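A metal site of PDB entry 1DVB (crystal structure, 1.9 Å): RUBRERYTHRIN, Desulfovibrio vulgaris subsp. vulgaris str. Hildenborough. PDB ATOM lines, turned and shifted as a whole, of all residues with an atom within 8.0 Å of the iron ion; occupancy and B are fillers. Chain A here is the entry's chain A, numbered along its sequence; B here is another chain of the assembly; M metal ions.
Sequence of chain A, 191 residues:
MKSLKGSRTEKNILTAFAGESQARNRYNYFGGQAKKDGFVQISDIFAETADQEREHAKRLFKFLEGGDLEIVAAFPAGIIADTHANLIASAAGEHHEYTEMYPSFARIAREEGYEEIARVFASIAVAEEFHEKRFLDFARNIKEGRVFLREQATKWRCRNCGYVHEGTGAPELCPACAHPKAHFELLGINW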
ATOM      1  N   ARG A 157     -15.792  23.491 -21.837  1.00  0.00           N
ATOM      2  CA  ARG A 157     -14.347  23.290 -21.889  1.00  0.00           C
ATOM      3  C   ARG A 157     -14.057  21.774 -21.926  1.00  0.00           C
ATOM      4  O   ARG A 157     -14.629  20.917 -21.276  1.00  0.00           O
ATOM      5  CB  ARG A 157     -13.668  24.020 -20.730  1.00  0.00           C
ATOM      6  CG  ARG A 157     -12.153  24.149 -20.850  1.00  0.00           C
ATOM      7  CD  ARG A 157     -11.509  24.547 -19.531  1.00  0.00           C
ATOM      8  NE  ARG A 157     -11.688  23.504 -18.511  1.00  0.00           N
ATOM      9  CZ  ARG A 157     -10.717  23.092 -17.701  1.00  0.00           C
ATOM     10  NH1 ARG A 157      -9.487  23.589 -17.768  1.00  0.00           N
ATOM     11  NH2 ARG A 157     -10.907  22.141 -16.786  1.00  0.00           N
ATOM     12  N   CYS A 158     -13.099  21.477 -22.780  1.00  0.00           N
ATOM     13  CA  CYS A 158     -12.420  20.203 -22.910  1.00  0.00           C
ATOM     14  C   CYS A 158     -11.477  20.037 -21.711  1.00  0.00           C
ATOM     15  O   CYS A 158     -10.542  20.816 -21.465  1.00  0.00           O
ATOM     16  CB  CYS A 158     -11.615  20.129 -24.197  1.00  0.00           C
ATOM     17  SG  CYS A 158     -10.901  18.486 -24.440  1.00  0.00           S
ATOM     18  N   ARG A 159     -11.773  18.965 -20.946  1.00  0.00           N
ATOM     19  CA  ARG A 159     -10.945  18.693 -19.771  1.00  0.00           C
ATOM     20  C   ARG A 159      -9.601  18.166 -20.245  1.00  0.00           C
ATOM     21  O   ARG A 159      -8.601  18.368 -19.568  1.00  0.00           O
ATOM     22  CB  ARG A 159     -11.650  17.719 -18.847  1.00  0.00           C
ATOM     23  CG  ARG A 159     -12.911  18.409 -18.310  1.00  0.00           C
ATOM     24  CD  ARG A 159     -13.500  17.793 -17.073  1.00  0.00           C
ATOM     25  NE  ARG A 159     -12.777  18.351 -15.861  1.00  0.00           N
ATOM     26  CZ  ARG A 159     -12.200  17.336 -15.221  1.00  0.00           C
ATOM     27  NH1 ARG A 159     -12.440  16.177 -15.846  1.00  0.00           N
ATOM     28  NH2 ARG A 159     -11.483  17.443 -14.147  1.00  0.00           N
ATOM     29  N   ASN A 160      -9.640  17.532 -21.413  1.00  0.00           N
ATOM     30  CA  ASN A 160      -8.394  16.905 -21.841  1.00  0.00           C
ATOM     31  C   ASN A 160      -7.339  17.890 -22.335  1.00  0.00           C
ATOM     32  O   ASN A 160      -6.146  17.689 -21.980  1.00  0.00           O
ATOM     33  CB  ASN A 160      -8.728  15.884 -22.935  1.00  0.00           C
ATOM     34  CG  ASN A 160      -7.500  15.017 -23.257  1.00  0.00           C
ATOM     35  OD1 ASN A 160      -6.814  14.555 -22.343  1.00  0.00           O
ATOM     36  ND2 ASN A 160      -7.296  14.867 -24.563  1.00  0.00           N
ATOM     37  N   CYS A 161      -7.747  18.914 -23.107  1.00  0.00           N
ATOM     38  CA  CYS A 161      -6.814  19.864 -23.671  1.00  0.00           C
ATOM     39  C   CYS A 161      -7.197  21.322 -23.434  1.00  0.00           C
ATOM     40  O   CYS A 161      -6.353  22.086 -23.940  1.00  0.00           O
ATOM     41  CB  CYS A 161      -6.649  19.799 -25.202  1.00  0.00           C
ATOM     42  SG  CYS A 161      -8.102  20.262 -26.143  1.00  0.00           S
ATOM     43  N   GLY A 162      -8.283  21.677 -22.791  1.00  0.00           N
ATOM     44  CA  GLY A 162      -8.522  23.104 -22.535  1.00  0.00           C
ATOM     45  C   GLY A 162      -9.269  23.836 -23.636  1.00  0.00           C
ATOM     46  O   GLY A 162      -9.543  25.040 -23.596  1.00  0.00           O
ATOM     47  N   TYR A 163      -9.623  23.058 -24.681  1.00  0.00           N
ATOM     48  CA  TYR A 163     -10.272  23.703 -25.790  1.00  0.00           C
ATOM     49  C   TYR A 163     -11.616  24.272 -25.318  1.00  0.00           C
ATOM     50  O   TYR A 163     -12.270  23.506 -24.604  1.00  0.00           O
ATOM     51  CB  TYR A 163     -10.557  22.752 -26.930  1.00  0.00           C
ATOM     52  CG  TYR A 163     -11.313  23.419 -28.063  1.00  0.00           C
ATOM     53  CD1 TYR A 163     -10.728  24.371 -28.895  1.00  0.00           C
ATOM     54  CD2 TYR A 163     -12.642  23.081 -28.304  1.00  0.00           C
ATOM     55  CE1 TYR A 163     -11.397  24.989 -29.924  1.00  0.00           C
ATOM     56  CE2 TYR A 163     -13.326  23.685 -29.341  1.00  0.00           C
ATOM     57  CZ  TYR A 163     -12.700  24.624 -30.121  1.00  0.00           C
ATOM     58  OH  TYR A 163     -13.426  25.191 -31.128  1.00  0.00           O
ATOM     59  N   VAL A 164     -11.889  25.498 -25.746  1.00  0.00           N
ATOM     60  CA  VAL A 164     -13.184  26.105 -25.354  1.00  0.00           C
ATOM     61  C   VAL A 164     -14.086  26.224 -26.592  1.00  0.00           C
ATOM     62  O   VAL A 164     -13.660  26.606 -27.663  1.00  0.00           O
ATOM     63  CB  VAL A 164     -12.973  27.435 -24.619  1.00  0.00           C
ATOM     64  CG1 VAL A 164     -14.301  28.065 -24.263  1.00  0.00           C
ATOM     65  CG2 VAL A 164     -12.172  27.228 -23.341  1.00  0.00           C
ATOM     66  N   PRO A 171     -19.277  19.620 -28.242  1.00  0.00           N
ATOM     67  CA  PRO A 171     -19.091  19.005 -29.564  1.00  0.00           C
ATOM     68  C   PRO A 171     -19.069  17.493 -29.534  1.00  0.00           C
ATOM     69  O   PRO A 171     -18.822  16.897 -28.484  1.00  0.00           O
ATOM     70  CB  PRO A 171     -17.681  19.480 -29.952  1.00  0.00           C
ATOM     71  CG  PRO A 171     -16.983  19.868 -28.696  1.00  0.00           C
ATOM     72  CD  PRO A 171     -18.070  20.311 -27.753  1.00  0.00           C
ATOM     73  N   LEU A 173     -16.773  15.542 -30.593  1.00  0.00           N
ATOM     74  CA  LEU A 173     -15.350  15.340 -30.759  1.00  0.00           C
ATOM     75  C   LEU A 173     -14.575  16.610 -30.501  1.00  0.00           C
ATOM     76  O   LEU A 173     -14.926  17.677 -31.027  1.00  0.00           O
ATOM     77  CB  LEU A 173     -15.130  14.883 -32.196  1.00  0.00           C
ATOM     78  CG  LEU A 173     -14.180  13.783 -32.615  1.00  0.00           C
ATOM     79  CD1 LEU A 173     -13.247  14.259 -33.726  1.00  0.00           C
ATOM     80  CD2 LEU A 173     -13.353  13.292 -31.434  1.00  0.00           C
ATOM     81  N   CYS A 174     -13.518  16.575 -29.704  1.00  0.00           N
ATOM     82  CA  CYS A 174     -12.830  17.852 -29.575  1.00  0.00           C
ATOM     83  C   CYS A 174     -12.039  18.173 -30.857  1.00  0.00           C
ATOM     84  O   CYS A 174     -11.217  17.407 -31.403  1.00  0.00           O
ATOM     85  CB  CYS A 174     -11.916  17.825 -28.342  1.00  0.00           C
ATOM     86  SG  CYS A 174     -11.030  19.372 -28.098  1.00  0.00           S
ATOM     87  N   PRO A 175     -12.280  19.379 -31.425  1.00  0.00           N
ATOM     88  CA  PRO A 175     -11.543  19.835 -32.594  1.00  0.00           C
ATOM     89  C   PRO A 175     -10.026  19.926 -32.322  1.00  0.00           C
ATOM     90  O   PRO A 175      -9.233  19.691 -33.232  1.00  0.00           O
ATOM     91  CB  PRO A 175     -12.083  21.234 -32.880  1.00  0.00           C
ATOM     92  CG  PRO A 175     -13.124  21.534 -31.864  1.00  0.00           C
ATOM     93  CD  PRO A 175     -13.290  20.346 -30.963  1.00  0.00           C
ATOM     94  N   ALA A 176      -9.630  20.266 -31.096  1.00  0.00           N
ATOM     95  CA  ALA A 176      -8.201  20.361 -30.761  1.00  0.00           C
ATOM     96  C   ALA A 176      -7.583  18.993 -30.469  1.00  0.00           C
ATOM     97  O   ALA A 176      -6.579  18.685 -31.116  1.00  0.00           O
ATOM     98  CB  ALA A 176      -7.965  21.325 -29.594  1.00  0.00           C
ATOM     99  N   CYS A 177      -8.106  18.186 -29.545  1.00  0.00           N
ATOM    100  CA  CYS A 177      -7.446  16.945 -29.146  1.00  0.00           C
ATOM    101  C   CYS A 177      -8.145  15.726 -29.675  1.00  0.00           C
ATOM    102  O   CYS A 177      -7.654  14.597 -29.526  1.00  0.00           O
ATOM    103  CB  CYS A 177      -7.352  16.936 -27.607  1.00  0.00           C
ATOM    104  SG  CYS A 177      -8.924  16.518 -26.806  1.00  0.00           S
ATOM    105  N   ALA A 178      -9.296  15.901 -30.333  1.00  0.00           N
ATOM    106  CA  ALA A 178      -9.997  14.757 -30.915  1.00  0.00           C
ATOM    107  C   ALA A 178     -10.468  13.719 -29.900  1.00  0.00           C
ATOM    108  O   ALA A 178     -10.761  12.548 -30.199  1.00  0.00           O
ATOM    109  CB  ALA A 178      -9.135  14.073 -31.976  1.00  0.00           C
ATOM    110  N   HIS A 179     -10.580  14.114 -28.628  1.00  0.00           N
ATOM    111  CA  HIS A 179     -11.250  13.272 -27.641  1.00  0.00           C
ATOM    112  C   HIS A 179     -12.759  13.525 -27.756  1.00  0.00           C
ATOM    113  O   HIS A 179     -13.285  14.545 -28.218  1.00  0.00           O
ATOM    114  CB  HIS A 179     -10.660  13.541 -26.273  1.00  0.00           C
ATOM    115  CG  HIS A 179      -9.314  12.912 -26.104  1.00  0.00           C
ATOM    116  ND1 HIS A 179      -8.273  13.110 -26.985  1.00  0.00           N
ATOM    117  CD2 HIS A 179      -8.821  12.086 -25.150  1.00  0.00           C
ATOM    118  CE1 HIS A 179      -7.191  12.444 -26.606  1.00  0.00           C
ATOM    119  NE2 HIS A 179      -7.510  11.810 -25.498  1.00  0.00           N
ATOM    120  N   PRO A 180     -13.571  12.552 -27.365  1.00  0.00           N
ATOM    121  CA  PRO A 180     -15.030  12.687 -27.487  1.00  0.00           C
ATOM    122  C   PRO A 180     -15.678  13.568 -26.413  1.00  0.00           C
ATOM    123  O   PRO A 180     -15.078  14.009 -25.445  1.00  0.00           O
ATOM    124  CB  PRO A 180     -15.542  11.241 -27.299  1.00  0.00           C
ATOM    125  CG  PRO A 180     -14.424  10.460 -26.714  1.00  0.00           C
ATOM    126  CD  PRO A 180     -13.156  11.259 -26.818  1.00  0.00           C
ATOM    127  N   HIS A 183     -15.392  14.336 -22.500  1.00  0.00           N
ATOM    128  CA  HIS A 183     -14.363  15.134 -21.843  1.00  0.00           C
ATOM    129  C   HIS A 183     -14.772  16.560 -21.534  1.00  0.00           C
ATOM    130  O   HIS A 183     -14.072  17.292 -20.814  1.00  0.00           O
ATOM    131  CB  HIS A 183     -13.107  15.106 -22.758  1.00  0.00           C
ATOM    132  CG  HIS A 183     -12.492  13.732 -22.692  1.00  0.00           C
ATOM    133  ND1 HIS A 183     -11.490  13.437 -21.789  1.00  0.00           N
ATOM    134  CD2 HIS A 183     -12.746  12.597 -23.382  1.00  0.00           C
ATOM    135  CE1 HIS A 183     -11.142  12.157 -21.945  1.00  0.00           C
ATOM    136  NE2 HIS A 183     -11.876  11.621 -22.903  1.00  0.00           N
ATOM    137  N   PHE A 184     -15.911  16.958 -22.090  1.00  0.00           N
ATOM    138  CA  PHE A 184     -16.345  18.364 -21.922  1.00  0.00           C
ATOM    139  C   PHE A 184     -17.126  18.661 -20.661  1.00  0.00           C
ATOM    140  O   PHE A 184     -17.862  17.821 -20.135  1.00  0.00           O
ATOM    141  CB  PHE A 184     -17.211  18.748 -23.153  1.00  0.00           C
ATOM    142  CG  PHE A 184     -16.276  19.114 -24.315  1.00  0.00           C
ATOM    143  CD1 PHE A 184     -15.775  20.408 -24.409  1.00  0.00           C
ATOM    144  CD2 PHE A 184     -15.947  18.128 -25.246  1.00  0.00           C
ATOM    145  CE1 PHE A 184     -14.925  20.746 -25.443  1.00  0.00           C
ATOM    146  CE2 PHE A 184     -15.090  18.458 -26.293  1.00  0.00           C
ATOM    147  CZ  PHE A 184     -14.606  19.750 -26.373  1.00  0.00           C
ATOM    148  N   GLN B  52      -2.511  19.529 -20.160  1.00  0.00           N
ATOM    149  CA  GLN B  52      -3.157  19.892 -21.451  1.00  0.00           C
ATOM    150  C   GLN B  52      -2.094  20.152 -22.513  1.00  0.00           C
ATOM    151  O   GLN B  52      -2.339  19.860 -23.668  1.00  0.00           O
ATOM    152  CB  GLN B  52      -4.098  21.069 -21.228  1.00  0.00           C
ATOM    153  CG  GLN B  52      -5.268  20.549 -20.358  1.00  0.00           C
ATOM    154  CD  GLN B  52      -6.301  21.614 -19.953  1.00  0.00           C
ATOM    155  OE1 GLN B  52      -5.982  22.820 -19.889  1.00  0.00           O
ATOM    156  NE2 GLN B  52      -7.519  21.155 -19.690  1.00  0.00           N
ATOM    157  N   GLU B  55      -1.202  17.145 -24.191  1.00  0.00           N
ATOM    158  CA  GLU B  55      -2.187  16.571 -25.122  1.00  0.00           C
ATOM    159  C   GLU B  55      -2.263  17.346 -26.421  1.00  0.00           C
ATOM    160  O   GLU B  55      -2.625  16.860 -27.476  1.00  0.00           O
ATOM    161  CB  GLU B  55      -3.538  16.487 -24.373  1.00  0.00           C
ATOM    162  CG  GLU B  55      -3.475  15.629 -23.105  1.00  0.00           C
ATOM    163  CD  GLU B  55      -3.374  14.158 -23.530  1.00  0.00           C
ATOM    164  OE1 GLU B  55      -4.005  13.822 -24.540  1.00  0.00           O
ATOM    165  OE2 GLU B  55      -2.659  13.380 -22.866  1.00  0.00           O
ATOM    166  N   HIS B  56      -1.906  18.622 -26.439  1.00  0.00           N
ATOM    167  CA  HIS B  56      -1.754  19.339 -27.689  1.00  0.00           C
ATOM    168  C   HIS B  56      -0.552  18.716 -28.436  1.00  0.00           C
ATOM    169  O   HIS B  56      -0.599  18.467 -29.627  1.00  0.00           O
ATOM    170  CB  HIS B  56      -1.465  20.824 -27.507  1.00  0.00           C
ATOM    171  CG  HIS B  56      -2.513  21.571 -26.793  1.00  0.00           C
ATOM    172  ND1 HIS B  56      -2.287  22.747 -26.127  1.00  0.00           N
ATOM    173  CD2 HIS B  56      -3.836  21.306 -26.656  1.00  0.00           C
ATOM    174  CE1 HIS B  56      -3.427  23.167 -25.594  1.00  0.00           C
ATOM    175  NE2 HIS B  56      -4.387  22.308 -25.906  1.00  0.00           N
ATOM    176  N   ARG B  59      -1.536  15.358 -30.172  1.00  0.00           N
ATOM    177  CA  ARG B  59      -2.243  15.409 -31.460  1.00  0.00           C
ATOM    178  C   ARG B  59      -1.289  15.809 -32.574  1.00  0.00           C
ATOM    179  O   ARG B  59      -1.327  15.249 -33.669  1.00  0.00           O
ATOM    180  CB  ARG B  59      -3.394  16.412 -31.358  1.00  0.00           C
ATOM    181  CG  ARG B  59      -4.244  16.633 -32.580  1.00  0.00           C
ATOM    182  CD  ARG B  59      -5.062  15.436 -32.977  1.00  0.00           C
ATOM    183  NE  ARG B  59      -6.252  15.596 -33.741  1.00  0.00           N
ATOM    184  CZ  ARG B  59      -7.165  16.525 -33.949  1.00  0.00           C
ATOM    185  NH1 ARG B  59      -7.131  17.698 -33.342  1.00  0.00           N
ATOM    186  NH2 ARG B  59      -8.167  16.268 -34.785  1.00  0.00           N
ATOM    187  N   SER B 123      -7.530  25.370 -33.501  1.00  0.00           N
ATOM    188  CA  SER B 123      -8.218  24.978 -32.256  1.00  0.00           C
ATOM    189  C   SER B 123      -7.303  25.084 -31.080  1.00  0.00           C
ATOM    190  O   SER B 123      -7.653  25.625 -30.032  1.00  0.00           O
ATOM    191  CB  SER B 123      -8.743  23.572 -32.482  1.00  0.00           C
ATOM    192  OG  SER B 123      -9.612  23.744 -33.595  1.00  0.00           O
ATOM    193  N   ALA B 127      -7.392  27.253 -27.068  1.00  0.00           N
ATOM    194  CA  ALA B 127      -7.017  26.781 -25.740  1.00  0.00           C
ATOM    195  C   ALA B 127      -5.951  27.662 -25.143  1.00  0.00           C
ATOM    196  O   ALA B 127      -5.989  27.983 -23.958  1.00  0.00           O
ATOM    197  CB  ALA B 127      -6.491  25.332 -25.770  1.00  0.00           C
HETATM  198 FE    FE M   1      -9.666  18.693 -26.360  1.00  0.00          FE
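The iron ion is bound by SG of Cys 161 (2.2 Å). SG of Cys 158 is bound to the iron ion, at 2.3 Å. SG of Cys 174 binds the iron ion, 2.3 Å away. The iron ion is bound by SG of Cys 177 (2.3 Å). The iron ion has four donor atoms within binding distance.
N of Tyr 163 lies close to SG of Cys 161 (3.5 Å). A ring nitrogen (NE2) of His 56 of chain B is in hydrogen-bond range of the backbone carbonyl oxygen (O) of Cys 161 (2.8 Å). The backbone NH (N) of Cys 158 lies within hydrogen-bond range of the backbone carbonyl oxygen (O) of Tyr 163 (2.9 Å). The side-chain sulfur (SG) of Cys 158 lies close to the backbone NH (N) of Asn 160 (3.4 Å). SG of Cys 174 lies close to N of Ala 176 (3.4 Å). The backbone carbonyl oxygen (O) of His 179 is in hydrogen-bond range of the backbone NH (N) of Cys 174, at 2.5 Å. ND2 of Asn 160 sits close to SG of Cys 177 (3.2 Å). O of Cys 177 sits at hydrogen-bond distance from ND1 of His 179 (3.0 Å).
Of the 25 residues printed, 4 come within 4 Å of the iron ion.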
